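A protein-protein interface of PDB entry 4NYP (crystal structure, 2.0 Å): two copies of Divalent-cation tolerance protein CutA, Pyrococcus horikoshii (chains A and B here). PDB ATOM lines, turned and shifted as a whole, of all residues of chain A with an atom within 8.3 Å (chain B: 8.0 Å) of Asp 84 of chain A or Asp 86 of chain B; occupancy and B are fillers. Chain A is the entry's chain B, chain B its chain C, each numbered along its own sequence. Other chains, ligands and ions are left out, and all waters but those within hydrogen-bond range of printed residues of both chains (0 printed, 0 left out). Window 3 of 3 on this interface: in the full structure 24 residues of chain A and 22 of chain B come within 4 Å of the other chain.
The indole nitrogen of Trp 62 of chain A is in hydrogen-bond range of the side-chain carboxylate of Asp 87 of chain B (2.8 Å). The backbone carbonyl oxygen of Arg 82 of chain A is in hydrogen-bond range of the backbone NH of Asp 86 of chain B (2.9 Å). N of Arg 82 of chain A sits at hydrogen-bond distance from O of Asp 87 of chain B, 2.8 Å away. The side-chain carboxylate (OD2) of Asp 86 of chain B sits at hydrogen-bond distance from the backbone NH (N) of Asp 84 of chain A, 2.7 Å away.
CZ2 of Trp 62 of chain A touches N of Val 88 of chain B, 3.9 Å away. CA of Val 88 of chain B touches O of Ile 80 of chain A (3.2 Å). CG1 of Val 85 of chain B touches CG2 of Ile 81 of chain A, at 3.6 Å. O of Asp 87 of chain B touches C of Ile 81 of chain A (3.8 Å). CG1 of Ile 81 of chain A touches CG2 of Val 88 of chain B, 3.999 Å away. Arg 82 of chain A touches Val 85 of chain B. Ile 83 of chain A touches Asp 86 of chain B (CA to OD2, 3.4 Å).
Of the 9 printed residues of chain B, 4 touch a printed residue of chain A. Printed residues of chain B that touch a printed residue of chain A: Val 85, Asp 86, Asp 87 and Val 88. Hydrophobic or aromatic side chains of chain B that line the printed part of chain A: Val 85 and Val 88.
N of Ile 83 of chain A lies within hydrogen-bond range of O of Ile 3 of chain A (2.9 Å). The side-chain carboxylate (OE2) of Glu 59 of chain A lies within salt-bridge range of the guanidinium group (NH2) of Arg 82 of chain A (3.4 Å). NE of Arg 82 of chain A is in salt-bridge range of OD1 of Asp 84 of chain A, at 2.8 Å. The backbone carbonyl oxygen (O) of Met 1 of chain B lies within hydrogen-bond range of the backbone NH (N) of Val 85 of chain B.
Ile 83 of chain A touches Asp 86 of chain B, but with the chains exchanged Asp 86 of chain A does not touch Ile 83 of chain B (7.3 Å). Asp 84 of chain A touches Asp 86 of chain B, but with the chains exchanged Asp 86 of chain A does not touch Asp 84 of chain B (8.0 Å). 8 positions are printed for both chains. Of the 11 pairs that touch across the chains among the printed residues, none has its exchanged pair printed and touching as well.
Asp 86 of chain B touches just these residues of chain A: Arg 82 (2.9 Å), Ile 83 (3.4 Å) and Asp 84 (2.7 Å). Of the printed residues of chain B, Arg 82 of chain A touches Val 85, Asp 86 and Asp 87. Of the printed residues of chain B, Ile 80 of chain A touches Val 88. Printed residues of chain B within 4 Å of Ile 81 of chain A: Val 85, Asp 87 and Val 88. Of the printed residues of chain A, Asp 87 of chain B touches Trp 62, Ile 81 and Arg 82. Ile 2 of chain B touches none of the printed residues of chain A. Ile 83 of chain B touches none of the printed residues of chain A. The nearest printed residue of chain B that does not touch Ile 80 of chain A is Asp 87 of chain B (4.2 Å).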
ATOM      1  N   MET A   1      14.606 -25.473   6.561  1.00  0.00           N
ATOM      2  CA  MET A   1      14.226 -24.536   5.467  1.00  0.00           C
ATOM      3  C   MET A   1      14.653 -23.116   5.830  1.00  0.00           C
ATOM      4  O   MET A   1      15.043 -22.840   6.972  1.00  0.00           O
ATOM      5  CB  MET A   1      12.712 -24.575   5.223  1.00  0.00           C
ATOM      6  CG  MET A   1      11.882 -24.079   6.394  1.00  0.00           C
ATOM      7  SD  MET A   1      10.172 -23.775   5.935  1.00  0.00           S
ATOM      8  CE  MET A   1      10.324 -22.186   5.094  1.00  0.00           C
ATOM      9  N   ILE A   2      14.584 -22.221   4.850  1.00  0.00           N
ATOM     10  CA  ILE A   2      14.979 -20.836   5.066  1.00  0.00           C
ATOM     11  C   ILE A   2      13.991 -19.862   4.439  1.00  0.00           C
ATOM     12  O   ILE A   2      13.209 -20.219   3.563  1.00  0.00           O
ATOM     13  CB  ILE A   2      16.374 -20.540   4.451  1.00  0.00           C
ATOM     14  CG1 ILE A   2      16.312 -20.698   2.925  1.00  0.00           C
ATOM     15  CG2 ILE A   2      17.431 -21.476   5.042  1.00  0.00           C
ATOM     16  CD1 ILE A   2      17.584 -20.275   2.203  1.00  0.00           C
ATOM     17  N   ILE A   3      14.044 -18.626   4.906  1.00  0.00           N
ATOM     18  CA  ILE A   3      13.217 -17.552   4.390  1.00  0.00           C
ATOM     19  C   ILE A   3      14.238 -16.599   3.773  1.00  0.00           C
ATOM     20  O   ILE A   3      15.292 -16.353   4.361  1.00  0.00           O
ATOM     21  CB  ILE A   3      12.474 -16.796   5.523  1.00  0.00           C
ATOM     22  CG1 ILE A   3      11.403 -17.691   6.163  1.00  0.00           C
ATOM     23  CG2 ILE A   3      11.865 -15.514   4.977  1.00  0.00           C
ATOM     24  CD1 ILE A   3      10.212 -17.974   5.283  1.00  0.00           C
ATOM     25  N   VAL A   4      13.946 -16.092   2.586  1.00  0.00           N
ATOM     26  CA  VAL A   4      14.842 -15.154   1.923  1.00  0.00           C
ATOM     27  C   VAL A   4      14.049 -13.887   1.645  1.00  0.00           C
ATOM     28  O   VAL A   4      12.979 -13.929   1.034  1.00  0.00           O
ATOM     29  CB  VAL A   4      15.393 -15.734   0.602  1.00  0.00           C
ATOM     30  CG1 VAL A   4      16.273 -14.696  -0.112  1.00  0.00           C
ATOM     31  CG2 VAL A   4      16.207 -16.980   0.899  1.00  0.00           C
ATOM     32  N   THR A  57      12.377 -21.585   0.720  1.00  0.00           N
ATOM     33  CA  THR A  57      13.055 -22.669   0.023  1.00  0.00           C
ATOM     34  C   THR A  57      13.924 -23.479   0.975  1.00  0.00           C
ATOM     35  O   THR A  57      13.963 -23.209   2.176  1.00  0.00           O
ATOM     36  CB  THR A  57      13.945 -22.117  -1.104  1.00  0.00           C
ATOM     37  OG1 THR A  57      14.438 -23.201  -1.904  1.00  0.00           O
ATOM     38  CG2 THR A  57      15.127 -21.343  -0.510  1.00  0.00           C
ATOM     39  N   ARG A  58      14.618 -24.473   0.424  1.00  0.00           N
ATOM     40  CA  ARG A  58      15.504 -25.331   1.203  1.00  0.00           C
ATOM     41  C   ARG A  58      16.832 -24.641   1.483  1.00  0.00           C
ATOM     42  O   ARG A  58      17.285 -23.793   0.712  1.00  0.00           O
ATOM     43  CB  ARG A  58      15.790 -26.636   0.464  1.00  0.00           C
ATOM     44  CG  ARG A  58      14.565 -27.429   0.052  1.00  0.00           C
ATOM     45  CD  ARG A  58      14.966 -28.875  -0.195  1.00  0.00           C
ATOM     46  NE  ARG A  58      16.165 -28.972  -1.020  1.00  0.00           N
ATOM     47  CZ  ARG A  58      16.166 -29.170  -2.334  1.00  0.00           C
ATOM     48  NH1 ARG A  58      15.025 -29.300  -2.999  1.00  0.00           N
ATOM     49  NH2 ARG A  58      17.322 -29.243  -2.986  1.00  0.00           N
ATOM     50  N   GLU A  59      17.461 -25.030   2.584  1.00  0.00           N
ATOM     51  CA  GLU A  59      18.733 -24.456   2.970  1.00  0.00           C
ATOM     52  C   GLU A  59      19.827 -24.692   1.925  1.00  0.00           C
ATOM     53  O   GLU A  59      20.534 -23.758   1.539  1.00  0.00           O
ATOM     54  CB  GLU A  59      19.171 -25.044   4.307  1.00  0.00           C
ATOM     55  CG  GLU A  59      20.312 -24.302   4.953  1.00  0.00           C
ATOM     56  CD  GLU A  59      20.774 -24.971   6.225  1.00  0.00           C
ATOM     57  OE1 GLU A  59      19.905 -25.321   7.057  1.00  0.00           O
ATOM     58  OE2 GLU A  59      22.005 -25.139   6.391  1.00  0.00           O
ATOM     59  N   TRP A  62      20.343 -22.250  -0.935  1.00  0.00           N
ATOM     60  CA  TRP A  62      20.700 -20.859  -0.644  1.00  0.00           C
ATOM     61  C   TRP A  62      21.723 -20.220  -1.589  1.00  0.00           C
ATOM     62  O   TRP A  62      21.457 -19.163  -2.172  1.00  0.00           O
ATOM     63  CB  TRP A  62      21.199 -20.743   0.799  1.00  0.00           C
ATOM     64  CG  TRP A  62      21.866 -19.427   1.124  1.00  0.00           C
ATOM     65  CD1 TRP A  62      23.119 -19.252   1.637  1.00  0.00           C
ATOM     66  CD2 TRP A  62      21.312 -18.114   0.967  1.00  0.00           C
ATOM     67  NE1 TRP A  62      23.379 -17.913   1.811  1.00  0.00           N
ATOM     68  CE2 TRP A  62      22.288 -17.192   1.408  1.00  0.00           C
ATOM     69  CE3 TRP A  62      20.085 -17.626   0.496  1.00  0.00           C
ATOM     70  CZ2 TRP A  62      22.078 -15.808   1.392  1.00  0.00           C
ATOM     71  CZ3 TRP A  62      19.876 -16.249   0.480  1.00  0.00           C
ATOM     72  CH2 TRP A  62      20.869 -15.358   0.926  1.00  0.00           C
ATOM     73  N   ILE A  80      19.468  -9.418  -0.307  1.00  0.00           N
ATOM     74  CA  ILE A  80      19.131 -10.838  -0.402  1.00  0.00           C
ATOM     75  C   ILE A  80      19.455 -11.379   0.983  1.00  0.00           C
ATOM     76  O   ILE A  80      20.545 -11.896   1.226  1.00  0.00           O
ATOM     77  CB  ILE A  80      19.984 -11.561  -1.453  1.00  0.00           C
ATOM     78  CG1 ILE A  80      19.993 -10.761  -2.760  1.00  0.00           C
ATOM     79  CG2 ILE A  80      19.419 -12.954  -1.702  1.00  0.00           C
ATOM     80  CD1 ILE A  80      20.876 -11.358  -3.840  1.00  0.00           C
ATOM     81  N   ILE A  81      18.481 -11.250   1.881  1.00  0.00           N
ATOM     82  CA  ILE A  81      18.622 -11.632   3.283  1.00  0.00           C
ATOM     83  C   ILE A  81      18.080 -13.011   3.643  1.00  0.00           C
ATOM     84  O   ILE A  81      16.906 -13.304   3.418  1.00  0.00           O
ATOM     85  CB  ILE A  81      17.929 -10.556   4.166  1.00  0.00           C
ATOM     86  CG1 ILE A  81      18.633  -9.207   3.962  1.00  0.00           C
ATOM     87  CG2 ILE A  81      17.948 -10.965   5.636  1.00  0.00           C
ATOM     88  CD1 ILE A  81      17.875  -8.021   4.527  1.00  0.00           C
ATOM     89  N   ARG A  82      18.942 -13.846   4.225  1.00  0.00           N
ATOM     90  CA  ARG A  82      18.564 -15.201   4.620  1.00  0.00           C
ATOM     91  C   ARG A  82      18.354 -15.349   6.125  1.00  0.00           C
ATOM     92  O   ARG A  82      19.215 -14.988   6.928  1.00  0.00           O
ATOM     93  CB  ARG A  82      19.629 -16.219   4.172  1.00  0.00           C
ATOM     94  CG  ARG A  82      19.506 -17.581   4.874  1.00  0.00           C
ATOM     95  CD  ARG A  82      20.591 -18.565   4.451  1.00  0.00           C
ATOM     96  NE  ARG A  82      20.597 -19.748   5.311  1.00  0.00           N
ATOM     97  CZ  ARG A  82      21.428 -20.779   5.169  1.00  0.00           C
ATOM     98  NH1 ARG A  82      22.328 -20.783   4.192  1.00  0.00           N
ATOM     99  NH2 ARG A  82      21.367 -21.804   6.013  1.00  0.00           N
ATOM    100  N   ILE A  83      17.200 -15.890   6.491  1.00  0.00           N
ATOM    101  CA  ILE A  83      16.867 -16.133   7.885  1.00  0.00           C
ATOM    102  C   ILE A  83      16.465 -17.601   8.003  1.00  0.00           C
ATOM    103  O   ILE A  83      15.515 -18.053   7.355  1.00  0.00           O
ATOM    104  CB  ILE A  83      15.708 -15.224   8.355  1.00  0.00           C
ATOM    105  CG1 ILE A  83      16.187 -13.766   8.406  1.00  0.00           C
ATOM    106  CG2 ILE A  83      15.221 -15.656   9.744  1.00  0.00           C
ATOM    107  CD1 ILE A  83      15.087 -12.783   8.730  1.00  0.00           C
ATOM    108  N   ASP A  84      17.216 -18.350   8.806  1.00  0.00           N
ATOM    109  CA  ASP A  84      16.936 -19.767   9.002  1.00  0.00           C
ATOM    110  C   ASP A  84      15.645 -19.968   9.788  1.00  0.00           C
ATOM    111  O   ASP A  84      15.344 -19.209  10.708  1.00  0.00           O
ATOM    112  CB  ASP A  84      18.092 -20.439   9.752  1.00  0.00           C
ATOM    113  CG  ASP A  84      19.343 -20.588   8.899  1.00  0.00           C
ATOM    114  OD1 ASP A  84      19.340 -20.164   7.729  1.00  0.00           O
ATOM    115  OD2 ASP A  84      20.342 -21.130   9.407  1.00  0.00           O
ATOM    116  N   VAL A  85      14.876 -20.984   9.413  1.00  0.00           N
ATOM    117  CA  VAL A  85      13.637 -21.300  10.119  1.00  0.00           C
ATOM    118  C   VAL A  85      14.010 -22.312  11.200  1.00  0.00           C
ATOM    119  O   VAL A  85      14.473 -23.410  10.896  1.00  0.00           O
ATOM    120  CB  VAL A  85      12.575 -21.905   9.161  1.00  0.00           C
ATOM    121  CG1 VAL A  85      11.410 -22.495   9.962  1.00  0.00           C
ATOM    122  CG2 VAL A  85      12.058 -20.821   8.221  1.00  0.00           C
ATOM    123  N   ASP A  86      13.825 -21.929  12.460  1.00  0.00           N
ATOM    124  CA  ASP A  86      14.170 -22.794  13.588  1.00  0.00           C
ATOM    125  C   ASP A  86      13.339 -24.070  13.673  1.00  0.00           C
ATOM    126  O   ASP A  86      13.807 -25.083  14.182  1.00  0.00           O
ATOM    127  CB  ASP A  86      14.073 -22.000  14.890  1.00  0.00           C
ATOM    128  CG  ASP A  86      15.058 -20.856  14.931  1.00  0.00           C
ATOM    129  OD1 ASP A  86      16.258 -21.115  15.163  1.00  0.00           O
ATOM    130  OD2 ASP A  86      14.634 -19.703  14.707  1.00  0.00           O
ATOM    131  N   ASP A  87      12.107 -24.015  13.187  1.00  0.00           N
ATOM    132  CA  ASP A  87      11.237 -25.191  13.168  1.00  0.00           C
ATOM    133  C   ASP A  87      10.026 -24.889  12.306  1.00  0.00           C
ATOM    134  O   ASP A  87       9.655 -23.722  12.123  1.00  0.00           O
ATOM    135  CB  ASP A  87      10.779 -25.584  14.577  1.00  0.00           C
ATOM    136  CG  ASP A  87      10.235 -27.009  14.633  1.00  0.00           C
ATOM    137  OD1 ASP A  87       9.596 -27.383  15.637  1.00  0.00           O
ATOM    138  OD2 ASP A  87      10.462 -27.765  13.670  1.00  0.00           O
ATOM    139  N   MET B   1      24.844  -9.128  10.213  1.00  0.00           N
ATOM    140  CA  MET B   1      23.859  -8.018  10.382  1.00  0.00           C
ATOM    141  C   MET B   1      22.616  -8.540  11.069  1.00  0.00           C
ATOM    142  O   MET B   1      22.429  -9.752  11.223  1.00  0.00           O
ATOM    143  CB  MET B   1      23.456  -7.431   9.023  1.00  0.00           C
ATOM    144  CG  MET B   1      22.694  -8.395   8.125  1.00  0.00           C
ATOM    145  SD  MET B   1      22.128  -7.658   6.584  1.00  0.00           S
ATOM    146  CE  MET B   1      20.720  -6.728   7.134  1.00  0.00           C
ATOM    147  N   ILE B   2      21.752  -7.618  11.468  1.00  0.00           N
ATOM    148  CA  ILE B   2      20.524  -7.999  12.128  1.00  0.00           C
ATOM    149  C   ILE B   2      19.368  -7.195  11.563  1.00  0.00           C
ATOM    150  O   ILE B   2      19.556  -6.170  10.897  1.00  0.00           O
ATOM    151  CB  ILE B   2      20.584  -7.724  13.646  1.00  0.00           C
ATOM    152  CG1 ILE B   2      20.827  -6.229  13.889  1.00  0.00           C
ATOM    153  CG2 ILE B   2      21.672  -8.565  14.294  1.00  0.00           C
ATOM    154  CD1 ILE B   2      20.723  -5.808  15.348  1.00  0.00           C
ATOM    155  N   GLU B  59      25.109  -5.913  14.169  1.00  0.00           N
ATOM    156  CA  GLU B  59      24.895  -6.531  15.472  1.00  0.00           C
ATOM    157  C   GLU B  59      25.457  -5.708  16.622  1.00  0.00           C
ATOM    158  O   GLU B  59      24.846  -5.622  17.683  1.00  0.00           O
ATOM    159  CB  GLU B  59      25.532  -7.924  15.522  1.00  0.00           C
ATOM    160  CG  GLU B  59      24.899  -8.939  14.592  1.00  0.00           C
ATOM    161  CD  GLU B  59      25.625  -9.066  13.270  1.00  0.00           C
ATOM    162  OE1 GLU B  59      26.055  -8.031  12.719  1.00  0.00           O
ATOM    163  OE2 GLU B  59      25.757 -10.207  12.776  1.00  0.00           O
ATOM    164  N   ILE B  83      16.240  -9.888  15.194  1.00  0.00           N
ATOM    165  CA  ILE B  83      16.346 -11.175  14.529  1.00  0.00           C
ATOM    166  C   ILE B  83      17.625 -11.153  13.717  1.00  0.00           C
ATOM    167  O   ILE B  83      17.786 -10.348  12.801  1.00  0.00           O
ATOM    168  CB  ILE B  83      15.132 -11.460  13.618  1.00  0.00           C
ATOM    169  CG1 ILE B  83      13.877 -11.624  14.485  1.00  0.00           C
ATOM    170  CG2 ILE B  83      15.384 -12.724  12.801  1.00  0.00           C
ATOM    171  CD1 ILE B  83      12.613 -11.964  13.731  1.00  0.00           C
ATOM    172  N   ASP B  84      18.543 -12.035  14.083  1.00  0.00           N
ATOM    173  CA  ASP B  84      19.826 -12.134  13.419  1.00  0.00           C
ATOM    174  C   ASP B  84      19.745 -12.689  12.006  1.00  0.00           C
ATOM    175  O   ASP B  84      19.024 -13.648  11.735  1.00  0.00           O
ATOM    176  CB  ASP B  84      20.767 -12.980  14.270  1.00  0.00           C
ATOM    177  CG  ASP B  84      21.270 -12.231  15.493  1.00  0.00           C
ATOM    178  OD1 ASP B  84      20.460 -11.560  16.160  1.00  0.00           O
ATOM    179  OD2 ASP B  84      22.476 -12.313  15.789  1.00  0.00           O
ATOM    180  N   VAL B  85      20.486 -12.064  11.100  1.00  0.00           N
ATOM    181  CA  VAL B  85      20.512 -12.499   9.715  1.00  0.00           C
ATOM    182  C   VAL B  85      21.551 -13.599   9.599  1.00  0.00           C
ATOM    183  O   VAL B  85      22.724 -13.392   9.900  1.00  0.00           O
ATOM    184  CB  VAL B  85      20.876 -11.336   8.773  1.00  0.00           C
ATOM    185  CG1 VAL B  85      21.020 -11.846   7.348  1.00  0.00           C
ATOM    186  CG2 VAL B  85      19.791 -10.262   8.842  1.00  0.00           C
ATOM    187  N   ASP B  86      21.111 -14.773   9.169  1.00  0.00           N
ATOM    188  CA  ASP B  86      22.004 -15.910   9.038  1.00  0.00           C
ATOM    189  C   ASP B  86      22.999 -15.758   7.897  1.00  0.00           C
ATOM    190  O   ASP B  86      24.148 -16.175   8.017  1.00  0.00           O
ATOM    191  CB  ASP B  86      21.170 -17.169   8.892  1.00  0.00           C
ATOM    192  CG  ASP B  86      20.365 -17.447  10.135  1.00  0.00           C
ATOM    193  OD1 ASP B  86      20.949 -17.976  11.095  1.00  0.00           O
ATOM    194  OD2 ASP B  86      19.163 -17.107  10.166  1.00  0.00           O
ATOM    195  N   ASP B  87      22.555 -15.183   6.788  1.00  0.00           N
ATOM    196  CA  ASP B  87      23.450 -14.928   5.670  1.00  0.00           C
ATOM    197  C   ASP B  87      22.823 -13.885   4.766  1.00  0.00           C
ATOM    198  O   ASP B  87      21.623 -13.625   4.845  1.00  0.00           O
ATOM    199  CB  ASP B  87      23.761 -16.204   4.882  1.00  0.00           C
ATOM    200  CG  ASP B  87      25.102 -16.118   4.145  1.00  0.00           C
ATOM    201  OD1 ASP B  87      25.452 -17.060   3.406  1.00  0.00           O
ATOM    202  OD2 ASP B  87      25.814 -15.102   4.315  1.00  0.00           O
ATOM    203  N   VAL B  88      23.641 -13.276   3.915  1.00  0.00           N
ATOM    204  CA  VAL B  88      23.160 -12.239   3.008  1.00  0.00           C
ATOM    205  C   VAL B  88      24.225 -11.980   1.941  1.00  0.00           C
ATOM    206  O   VAL B  88      25.407 -12.288   2.152  1.00  0.00           O
ATOM    207  CB  VAL B  88      22.854 -10.933   3.809  1.00  0.00           C
ATOM    208  CG1 VAL B  88      24.075 -10.528   4.617  1.00  0.00           C
ATOM    209  CG2 VAL B  88      22.434  -9.805   2.874  1.00  0.00           C
